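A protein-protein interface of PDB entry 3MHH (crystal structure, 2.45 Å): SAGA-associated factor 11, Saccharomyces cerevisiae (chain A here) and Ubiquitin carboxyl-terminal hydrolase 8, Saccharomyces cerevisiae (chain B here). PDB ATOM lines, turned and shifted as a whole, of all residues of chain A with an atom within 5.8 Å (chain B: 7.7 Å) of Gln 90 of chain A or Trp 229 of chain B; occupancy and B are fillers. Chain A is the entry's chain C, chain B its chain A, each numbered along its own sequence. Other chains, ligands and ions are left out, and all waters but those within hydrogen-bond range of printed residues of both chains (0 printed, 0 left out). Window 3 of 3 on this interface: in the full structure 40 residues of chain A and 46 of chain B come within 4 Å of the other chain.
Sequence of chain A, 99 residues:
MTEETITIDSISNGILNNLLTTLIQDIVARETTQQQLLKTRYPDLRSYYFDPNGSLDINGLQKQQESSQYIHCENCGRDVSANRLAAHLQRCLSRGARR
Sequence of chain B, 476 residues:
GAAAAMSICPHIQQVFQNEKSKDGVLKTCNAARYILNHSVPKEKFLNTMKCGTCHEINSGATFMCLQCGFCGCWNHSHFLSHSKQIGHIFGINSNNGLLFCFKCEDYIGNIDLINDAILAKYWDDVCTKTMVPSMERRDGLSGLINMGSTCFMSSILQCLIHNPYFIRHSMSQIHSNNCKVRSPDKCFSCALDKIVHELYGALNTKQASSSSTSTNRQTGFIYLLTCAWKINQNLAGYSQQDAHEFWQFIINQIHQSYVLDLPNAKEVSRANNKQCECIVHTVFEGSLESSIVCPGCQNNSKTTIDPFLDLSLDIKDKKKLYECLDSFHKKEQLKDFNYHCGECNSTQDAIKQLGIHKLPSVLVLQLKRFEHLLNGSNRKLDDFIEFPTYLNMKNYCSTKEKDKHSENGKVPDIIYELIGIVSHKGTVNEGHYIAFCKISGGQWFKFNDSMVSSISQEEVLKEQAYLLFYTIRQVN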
ATOM      1  N   LEU A  85      18.915  14.445  -9.640  1.00  0.00           N
ATOM      2  CA  LEU A  85      20.373  14.570  -9.759  1.00  0.00           C
ATOM      3  C   LEU A  85      21.064  14.838  -8.422  1.00  0.00           C
ATOM      4  O   LEU A  85      22.171  14.352  -8.198  1.00  0.00           O
ATOM      5  CB  LEU A  85      20.756  15.670 -10.753  1.00  0.00           C
ATOM      6  CG  LEU A  85      21.863  15.335 -11.763  1.00  0.00           C
ATOM      7  CD1 LEU A  85      22.686  16.568 -12.088  1.00  0.00           C
ATOM      8  CD2 LEU A  85      22.769  14.214 -11.287  1.00  0.00           C
ATOM      9  N   ALA A  86      20.430  15.619  -7.548  1.00  0.00           N
ATOM     10  CA  ALA A  86      21.021  15.953  -6.251  1.00  0.00           C
ATOM     11  C   ALA A  86      21.133  14.711  -5.370  1.00  0.00           C
ATOM     12  O   ALA A  86      22.181  14.442  -4.799  1.00  0.00           O
ATOM     13  CB  ALA A  86      20.210  17.025  -5.546  1.00  0.00           C
ATOM     14  N   ALA A  87      20.049  13.952  -5.266  1.00  0.00           N
ATOM     15  CA  ALA A  87      20.044  12.735  -4.462  1.00  0.00           C
ATOM     16  C   ALA A  87      21.005  11.716  -5.069  1.00  0.00           C
ATOM     17  O   ALA A  87      21.720  11.031  -4.360  1.00  0.00           O
ATOM     18  CB  ALA A  87      18.633  12.161  -4.370  1.00  0.00           C
ATOM     19  N   HIS A  88      21.048  11.651  -6.391  1.00  0.00           N
ATOM     20  CA  HIS A  88      21.930  10.703  -7.059  1.00  0.00           C
ATOM     21  C   HIS A  88      23.394  11.026  -6.764  1.00  0.00           C
ATOM     22  O   HIS A  88      24.174  10.145  -6.431  1.00  0.00           O
ATOM     23  CB  HIS A  88      21.671  10.692  -8.571  1.00  0.00           C
ATOM     24  CG  HIS A  88      22.673   9.891  -9.340  1.00  0.00           C
ATOM     25  ND1 HIS A  88      22.597   8.520  -9.456  1.00  0.00           N
ATOM     26  CD2 HIS A  88      23.798  10.266  -9.995  1.00  0.00           C
ATOM     27  CE1 HIS A  88      23.629   8.085 -10.160  1.00  0.00           C
ATOM     28  NE2 HIS A  88      24.383   9.124 -10.482  1.00  0.00           N
ATOM     29  N   LEU A  89      23.755  12.298  -6.884  1.00  0.00           N
ATOM     30  CA  LEU A  89      25.131  12.731  -6.635  1.00  0.00           C
ATOM     31  C   LEU A  89      25.594  12.297  -5.243  1.00  0.00           C
ATOM     32  O   LEU A  89      26.655  11.694  -5.111  1.00  0.00           O
ATOM     33  CB  LEU A  89      25.274  14.248  -6.825  1.00  0.00           C
ATOM     34  CG  LEU A  89      25.228  14.763  -8.271  1.00  0.00           C
ATOM     35  CD1 LEU A  89      25.404  16.284  -8.328  1.00  0.00           C
ATOM     36  CD2 LEU A  89      26.269  14.088  -9.154  1.00  0.00           C
ATOM     37  N   GLN A  90      24.789  12.560  -4.214  1.00  0.00           N
ATOM     38  CA  GLN A  90      25.149  12.153  -2.852  1.00  0.00           C
ATOM     39  C   GLN A  90      25.482  10.671  -2.747  1.00  0.00           C
ATOM     40  O   GLN A  90      26.347  10.287  -1.969  1.00  0.00           O
ATOM     41  CB  GLN A  90      24.039  12.508  -1.861  1.00  0.00           C
ATOM     42  CG  GLN A  90      24.279  13.824  -1.129  1.00  0.00           C
ATOM     43  CD  GLN A  90      23.025  14.667  -1.004  1.00  0.00           C
ATOM     44  OE1 GLN A  90      23.020  15.847  -1.366  1.00  0.00           O
ATOM     45  NE2 GLN A  90      21.948  14.061  -0.507  1.00  0.00           N
ATOM     46  N   ARG A  91      24.803   9.839  -3.527  1.00  0.00           N
ATOM     47  CA  ARG A  91      25.032   8.401  -3.496  1.00  0.00           C
ATOM     48  C   ARG A  91      26.089   7.942  -4.492  1.00  0.00           C
ATOM     49  O   ARG A  91      26.683   6.889  -4.321  1.00  0.00           O
ATOM     50  CB  ARG A  91      23.725   7.642  -3.761  1.00  0.00           C
ATOM     51  CG  ARG A  91      22.991   7.197  -2.502  1.00  0.00           C
ATOM     52  CD  ARG A  91      21.665   6.511  -2.825  1.00  0.00           C
ATOM     53  NE  ARG A  91      20.658   7.481  -3.257  1.00  0.00           N
ATOM     54  CZ  ARG A  91      20.344   7.726  -4.525  1.00  0.00           C
ATOM     55  NH1 ARG A  91      20.935   7.060  -5.509  1.00  0.00           N
ATOM     56  NH2 ARG A  91      19.421   8.625  -4.808  1.00  0.00           N
ATOM     57  N   CYS A  92      26.312   8.718  -5.540  1.00  0.00           N
ATOM     58  CA  CYS A  92      27.230   8.320  -6.603  1.00  0.00           C
ATOM     59  C   CYS A  92      28.659   8.763  -6.314  1.00  0.00           C
ATOM     60  O   CYS A  92      29.613   8.035  -6.570  1.00  0.00           O
ATOM     61  CB  CYS A  92      26.775   8.940  -7.918  1.00  0.00           C
ATOM     62  SG  CYS A  92      27.648   8.339  -9.346  1.00  0.00           S
ATOM     63  N   LEU A  93      28.798   9.975  -5.789  1.00  0.00           N
ATOM     64  CA  LEU A  93      30.108  10.544  -5.518  1.00  0.00           C
ATOM     65  C   LEU A  93      30.769   9.840  -4.335  1.00  0.00           C
ATOM     66  O   LEU A  93      31.984   9.905  -4.158  1.00  0.00           O
ATOM     67  CB  LEU A  93      29.977  12.049  -5.260  1.00  0.00           C
ATOM     68  CG  LEU A  93      29.510  12.857  -6.476  1.00  0.00           C
ATOM     69  CD1 LEU A  93      29.430  14.362  -6.162  1.00  0.00           C
ATOM     70  CD2 LEU A  93      30.439  12.608  -7.652  1.00  0.00           C
ATOM     71  N   SER A  94      29.958   9.164  -3.531  1.00  0.00           N
ATOM     72  CA  SER A  94      30.467   8.366  -2.424  1.00  0.00           C
ATOM     73  C   SER A  94      31.525   7.377  -2.928  1.00  0.00           C
ATOM     74  O   SER A  94      32.564   7.183  -2.286  1.00  0.00           O
ATOM     75  CB  SER A  94      29.314   7.610  -1.748  1.00  0.00           C
ATOM     76  OG  SER A  94      28.690   6.706  -2.649  1.00  0.00           O
ATOM     77  N   GLY B 148      16.210  18.262  -7.100  1.00  0.00           N
ATOM     78  CA  GLY B 148      15.853  17.583  -5.856  1.00  0.00           C
ATOM     79  C   GLY B 148      15.983  18.527  -4.685  1.00  0.00           C
ATOM     80  O   GLY B 148      16.985  18.514  -3.973  1.00  0.00           O
ATOM     81  N   THR B 150      16.540  21.843  -4.671  1.00  0.00           N
ATOM     82  CA  THR B 150      17.720  22.700  -4.833  1.00  0.00           C
ATOM     83  C   THR B 150      17.345  24.134  -5.261  1.00  0.00           C
ATOM     84  O   THR B 150      18.192  24.906  -5.703  1.00  0.00           O
ATOM     85  CB  THR B 150      18.709  22.088  -5.848  1.00  0.00           C
ATOM     86  OG1 THR B 150      18.099  22.026  -7.141  1.00  0.00           O
ATOM     87  CG2 THR B 150      19.114  20.679  -5.411  1.00  0.00           C
ATOM     88  N   MET B 153      19.112  26.897  -3.542  1.00  0.00           N
ATOM     89  CA  MET B 153      20.418  27.217  -4.100  1.00  0.00           C
ATOM     90  C   MET B 153      20.287  28.020  -5.384  1.00  0.00           C
ATOM     91  O   MET B 153      20.965  29.044  -5.559  1.00  0.00           O
ATOM     92  CB  MET B 153      21.189  25.932  -4.413  1.00  0.00           C
ATOM     93  CG  MET B 153      21.753  25.236  -3.195  1.00  0.00           C
ATOM     94  SD  MET B 153      22.401  23.598  -3.621  1.00  0.00           S
ATOM     95  CE  MET B 153      23.788  24.056  -4.655  1.00  0.00           C
ATOM     96  N   ASP B 185      34.810  21.123 -10.799  1.00  0.00           N
ATOM     97  CA  ASP B 185      34.254  20.043  -9.986  1.00  0.00           C
ATOM     98  C   ASP B 185      34.828  20.005  -8.561  1.00  0.00           C
ATOM     99  O   ASP B 185      34.434  19.149  -7.763  1.00  0.00           O
ATOM    100  CB  ASP B 185      34.413  18.677 -10.674  1.00  0.00           C
ATOM    101  CG  ASP B 185      35.808  18.449 -11.221  1.00  0.00           C
ATOM    102  OD1 ASP B 185      36.587  19.421 -11.305  1.00  0.00           O
ATOM    103  OD2 ASP B 185      36.121  17.298 -11.585  1.00  0.00           O
ATOM    104  N   PHE B 188      34.503  25.977  -5.866  1.00  0.00           N
ATOM    105  CA  PHE B 188      33.252  26.709  -5.991  1.00  0.00           C
ATOM    106  C   PHE B 188      33.374  27.885  -6.959  1.00  0.00           C
ATOM    107  O   PHE B 188      32.564  28.032  -7.885  1.00  0.00           O
ATOM    108  CB  PHE B 188      32.793  27.225  -4.632  1.00  0.00           C
ATOM    109  CG  PHE B 188      32.276  26.156  -3.732  1.00  0.00           C
ATOM    110  CD1 PHE B 188      30.931  25.818  -3.744  1.00  0.00           C
ATOM    111  CD2 PHE B 188      33.136  25.476  -2.878  1.00  0.00           C
ATOM    112  CE1 PHE B 188      30.452  24.807  -2.926  1.00  0.00           C
ATOM    113  CE2 PHE B 188      32.665  24.465  -2.047  1.00  0.00           C
ATOM    114  CZ  PHE B 188      31.323  24.128  -2.072  1.00  0.00           C
ATOM    115  N   TYR B 223      28.291  21.210 -11.544  1.00  0.00           N
ATOM    116  CA  TYR B 223      29.634  21.290 -10.977  1.00  0.00           C
ATOM    117  C   TYR B 223      29.578  21.849  -9.556  1.00  0.00           C
ATOM    118  O   TYR B 223      30.345  21.442  -8.687  1.00  0.00           O
ATOM    119  CB  TYR B 223      30.547  22.181 -11.834  1.00  0.00           C
ATOM    120  CG  TYR B 223      31.097  21.529 -13.080  1.00  0.00           C
ATOM    121  CD1 TYR B 223      31.702  20.280 -13.030  1.00  0.00           C
ATOM    122  CD2 TYR B 223      31.071  22.190 -14.298  1.00  0.00           C
ATOM    123  CE1 TYR B 223      32.225  19.687 -14.169  1.00  0.00           C
ATOM    124  CE2 TYR B 223      31.602  21.610 -15.440  1.00  0.00           C
ATOM    125  CZ  TYR B 223      32.176  20.357 -15.369  1.00  0.00           C
ATOM    126  OH  TYR B 223      32.708  19.784 -16.502  1.00  0.00           O
ATOM    127  N   LEU B 224      28.672  22.784  -9.323  1.00  0.00           N
ATOM    128  CA  LEU B 224      28.591  23.453  -8.027  1.00  0.00           C
ATOM    129  C   LEU B 224      28.027  22.490  -6.997  1.00  0.00           C
ATOM    130  O   LEU B 224      28.440  22.484  -5.836  1.00  0.00           O
ATOM    131  CB  LEU B 224      27.721  24.710  -8.120  1.00  0.00           C
ATOM    132  CG  LEU B 224      27.641  25.592  -6.865  1.00  0.00           C
ATOM    133  CD1 LEU B 224      27.028  26.952  -7.190  1.00  0.00           C
ATOM    134  CD2 LEU B 224      26.835  24.905  -5.746  1.00  0.00           C
ATOM    135  N   LEU B 225      27.072  21.673  -7.415  1.00  0.00           N
ATOM    136  CA  LEU B 225      26.535  20.653  -6.524  1.00  0.00           C
ATOM    137  C   LEU B 225      27.645  19.687  -6.151  1.00  0.00           C
ATOM    138  O   LEU B 225      27.792  19.309  -4.988  1.00  0.00           O
ATOM    139  CB  LEU B 225      25.389  19.897  -7.194  1.00  0.00           C
ATOM    140  CG  LEU B 225      24.076  20.666  -7.308  1.00  0.00           C
ATOM    141  CD1 LEU B 225      23.208  20.042  -8.365  1.00  0.00           C
ATOM    142  CD2 LEU B 225      23.375  20.695  -5.966  1.00  0.00           C
ATOM    143  N   THR B 226      28.444  19.312  -7.145  1.00  0.00           N
ATOM    144  CA  THR B 226      29.565  18.420  -6.917  1.00  0.00           C
ATOM    145  C   THR B 226      30.581  19.034  -5.938  1.00  0.00           C
ATOM    146  O   THR B 226      31.070  18.360  -5.023  1.00  0.00           O
ATOM    147  CB  THR B 226      30.233  18.032  -8.246  1.00  0.00           C
ATOM    148  OG1 THR B 226      29.249  17.456  -9.124  1.00  0.00           O
ATOM    149  CG2 THR B 226      31.356  17.028  -8.015  1.00  0.00           C
ATOM    150  N   CYS B 227      30.874  20.322  -6.102  1.00  0.00           N
ATOM    151  CA  CYS B 227      31.734  21.017  -5.149  1.00  0.00           C
ATOM    152  C   CYS B 227      31.120  20.976  -3.763  1.00  0.00           C
ATOM    153  O   CYS B 227      31.802  20.709  -2.777  1.00  0.00           O
ATOM    154  CB  CYS B 227      31.918  22.475  -5.558  1.00  0.00           C
ATOM    155  SG  CYS B 227      32.985  22.694  -6.957  1.00  0.00           S
ATOM    156  N   ALA B 228      29.828  21.280  -3.706  1.00  0.00           N
ATOM    157  CA  ALA B 228      29.096  21.338  -2.453  1.00  0.00           C
ATOM    158  C   ALA B 228      29.238  20.039  -1.709  1.00  0.00           C
ATOM    159  O   ALA B 228      29.542  20.033  -0.517  1.00  0.00           O
ATOM    160  CB  ALA B 228      27.635  21.627  -2.710  1.00  0.00           C
ATOM    161  N   TRP B 229      29.041  18.932  -2.414  1.00  0.00           N
ATOM    162  CA  TRP B 229      29.098  17.625  -1.781  1.00  0.00           C
ATOM    163  C   TRP B 229      30.476  17.315  -1.210  1.00  0.00           C
ATOM    164  O   TRP B 229      30.574  16.674  -0.164  1.00  0.00           O
ATOM    165  CB  TRP B 229      28.692  16.520  -2.757  1.00  0.00           C
ATOM    166  CG  TRP B 229      28.768  15.153  -2.143  1.00  0.00           C
ATOM    167  CD1 TRP B 229      27.783  14.511  -1.448  1.00  0.00           C
ATOM    168  CD2 TRP B 229      29.899  14.270  -2.144  1.00  0.00           C
ATOM    169  NE1 TRP B 229      28.225  13.280  -1.033  1.00  0.00           N
ATOM    170  CE2 TRP B 229      29.517  13.104  -1.450  1.00  0.00           C
ATOM    171  CE3 TRP B 229      31.190  14.347  -2.678  1.00  0.00           C
ATOM    172  CZ2 TRP B 229      30.386  12.028  -1.264  1.00  0.00           C
ATOM    173  CZ3 TRP B 229      32.048  13.272  -2.501  1.00  0.00           C
ATOM    174  CH2 TRP B 229      31.642  12.130  -1.797  1.00  0.00           C
ATOM    175  N   LYS B 230      31.533  17.735  -1.905  1.00  0.00           N
ATOM    176  CA  LYS B 230      32.905  17.469  -1.453  1.00  0.00           C
ATOM    177  C   LYS B 230      33.209  18.149  -0.113  1.00  0.00           C
ATOM    178  O   LYS B 230      33.991  17.645   0.688  1.00  0.00           O
ATOM    179  CB  LYS B 230      33.924  17.947  -2.488  1.00  0.00           C
ATOM    180  CG  LYS B 230      33.960  17.155  -3.780  1.00  0.00           C
ATOM    181  CD  LYS B 230      35.353  17.220  -4.403  1.00  0.00           C
ATOM    182  CE  LYS B 230      35.318  17.106  -5.923  1.00  0.00           C
ATOM    183  NZ  LYS B 230      34.512  15.957  -6.418  1.00  0.00           N
ATOM    184  N   ILE B 231      32.603  19.310   0.108  1.00  0.00           N
ATOM    185  CA  ILE B 231      32.770  20.053   1.356  1.00  0.00           C
ATOM    186  C   ILE B 231      31.665  19.701   2.354  1.00  0.00           C
ATOM    187  O   ILE B 231      31.866  19.782   3.565  1.00  0.00           O
ATOM    188  CB  ILE B 231      32.774  21.576   1.086  1.00  0.00           C
ATOM    189  CG1 ILE B 231      34.213  22.056   0.857  1.00  0.00           C
ATOM    190  CG2 ILE B 231      32.118  22.341   2.231  1.00  0.00           C
ATOM    191  CD1 ILE B 231      35.203  21.619   1.941  1.00  0.00           C
ATOM    192  N   ASN B 232      30.511  19.299   1.822  1.00  0.00           N
ATOM    193  CA  ASN B 232      29.366  18.841   2.613  1.00  0.00           C
ATOM    194  C   ASN B 232      28.578  20.020   3.194  1.00  0.00           C
ATOM    195  O   ASN B 232      27.881  20.739   2.471  1.00  0.00           O
ATOM    196  CB  ASN B 232      29.805  17.877   3.733  1.00  0.00           C
ATOM    197  CG  ASN B 232      30.813  16.826   3.257  1.00  0.00           C
ATOM    198  OD1 ASN B 232      30.667  15.636   3.538  1.00  0.00           O
ATOM    199  ND2 ASN B 232      31.848  17.271   2.553  1.00  0.00           N
ATOM    200  N   SER B 239      19.042  19.728   3.380  1.00  0.00           N
ATOM    201  CA  SER B 239      18.857  19.510   4.815  1.00  0.00           C
ATOM    202  C   SER B 239      17.834  20.496   5.396  1.00  0.00           C
ATOM    203  O   SER B 239      16.631  20.211   5.423  1.00  0.00           O
ATOM    204  CB  SER B 239      20.198  19.639   5.546  1.00  0.00           C
ATOM    205  OG  SER B 239      20.036  19.525   6.950  1.00  0.00           O
ATOM    206  N   PHE B 249      26.734  30.589   2.874  1.00  0.00           N
ATOM    207  CA  PHE B 249      27.671  29.535   2.559  1.00  0.00           C
ATOM    208  C   PHE B 249      28.517  29.923   1.359  1.00  0.00           C
ATOM    209  O   PHE B 249      29.728  29.828   1.391  1.00  0.00           O
ATOM    210  CB  PHE B 249      26.931  28.233   2.274  1.00  0.00           C
ATOM    211  CG  PHE B 249      27.801  27.166   1.707  1.00  0.00           C
ATOM    212  CD1 PHE B 249      28.480  26.290   2.541  1.00  0.00           C
ATOM    213  CD2 PHE B 249      27.946  27.035   0.336  1.00  0.00           C
ATOM    214  CE1 PHE B 249      29.292  25.299   2.017  1.00  0.00           C
ATOM    215  CE2 PHE B 249      28.758  26.049  -0.198  1.00  0.00           C
ATOM    216  CZ  PHE B 249      29.432  25.177   0.644  1.00  0.00           C
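Of the printed residues of chain B, Leu 89 of chain A touches Leu 225 (3.8 Å). Gln 90 of chain A touches one residue of chain B. Of the printed residues of chain B, Leu 93 of chain A touches Thr 226 (3.8 Å) and Trp 229 (3.3 Å). Asp 185 of chain B touches none of the printed residues of chain A. Of chain A, only Gln 90 (3.6 Å), Leu 93 (3.3 Å) and Ser 94 (3.7 Å) come within 4 Å of Trp 229 of chain B. Asn 232 of chain B touches none of the printed residues of chain A. The nearest residue of chain A that does not touch Trp 229 of chain B is Leu 89 of chain A (4.6 Å). The nearest printed residue of chain A that does not touch Thr 150 of chain B is Ala 87 of chain A (6.8 Å).
O of Trp 229 of chain B sits at hydrogen-bond distance from ND2 of Asn 232 of chain B, at 3.1 Å. O of Arg 91 of chain A lies within hydrogen-bond range of OG of Ser 94 of chain A, at 2.6 Å.
Among the printed residues, merely in contact across the chains: Leu 93 of chain A with Trp 229 of chain B (3.3 Å), Gln 90 of chain A with Trp 229 of chain B (3.6 Å), Ser 94 of chain A with Trp 229 of chain B (3.7 Å), Leu 93 of chain A with Thr 226 of chain B (3.8 Å), Leu 89 of chain A with Leu 225 of chain B (3.8 Å), Ala 86 of chain A with Thr 150 of chain B (3.8 Å) and Ala 86 of chain A with Gly 148 of chain B (3.9 Å).
Hydrophobic or aromatic side chains of chain B that line the printed part of chain A: Leu 225 and Trp 229. Printed residues of chain A that touch a printed residue of chain B: Ala 86, Leu 89, Gln 90, Leu 93 and Ser 94. Among the printed residues, no Asp or Glu carboxylate lies within 4 Å of a Lys or Arg side-chain nitrogen of the other chain.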
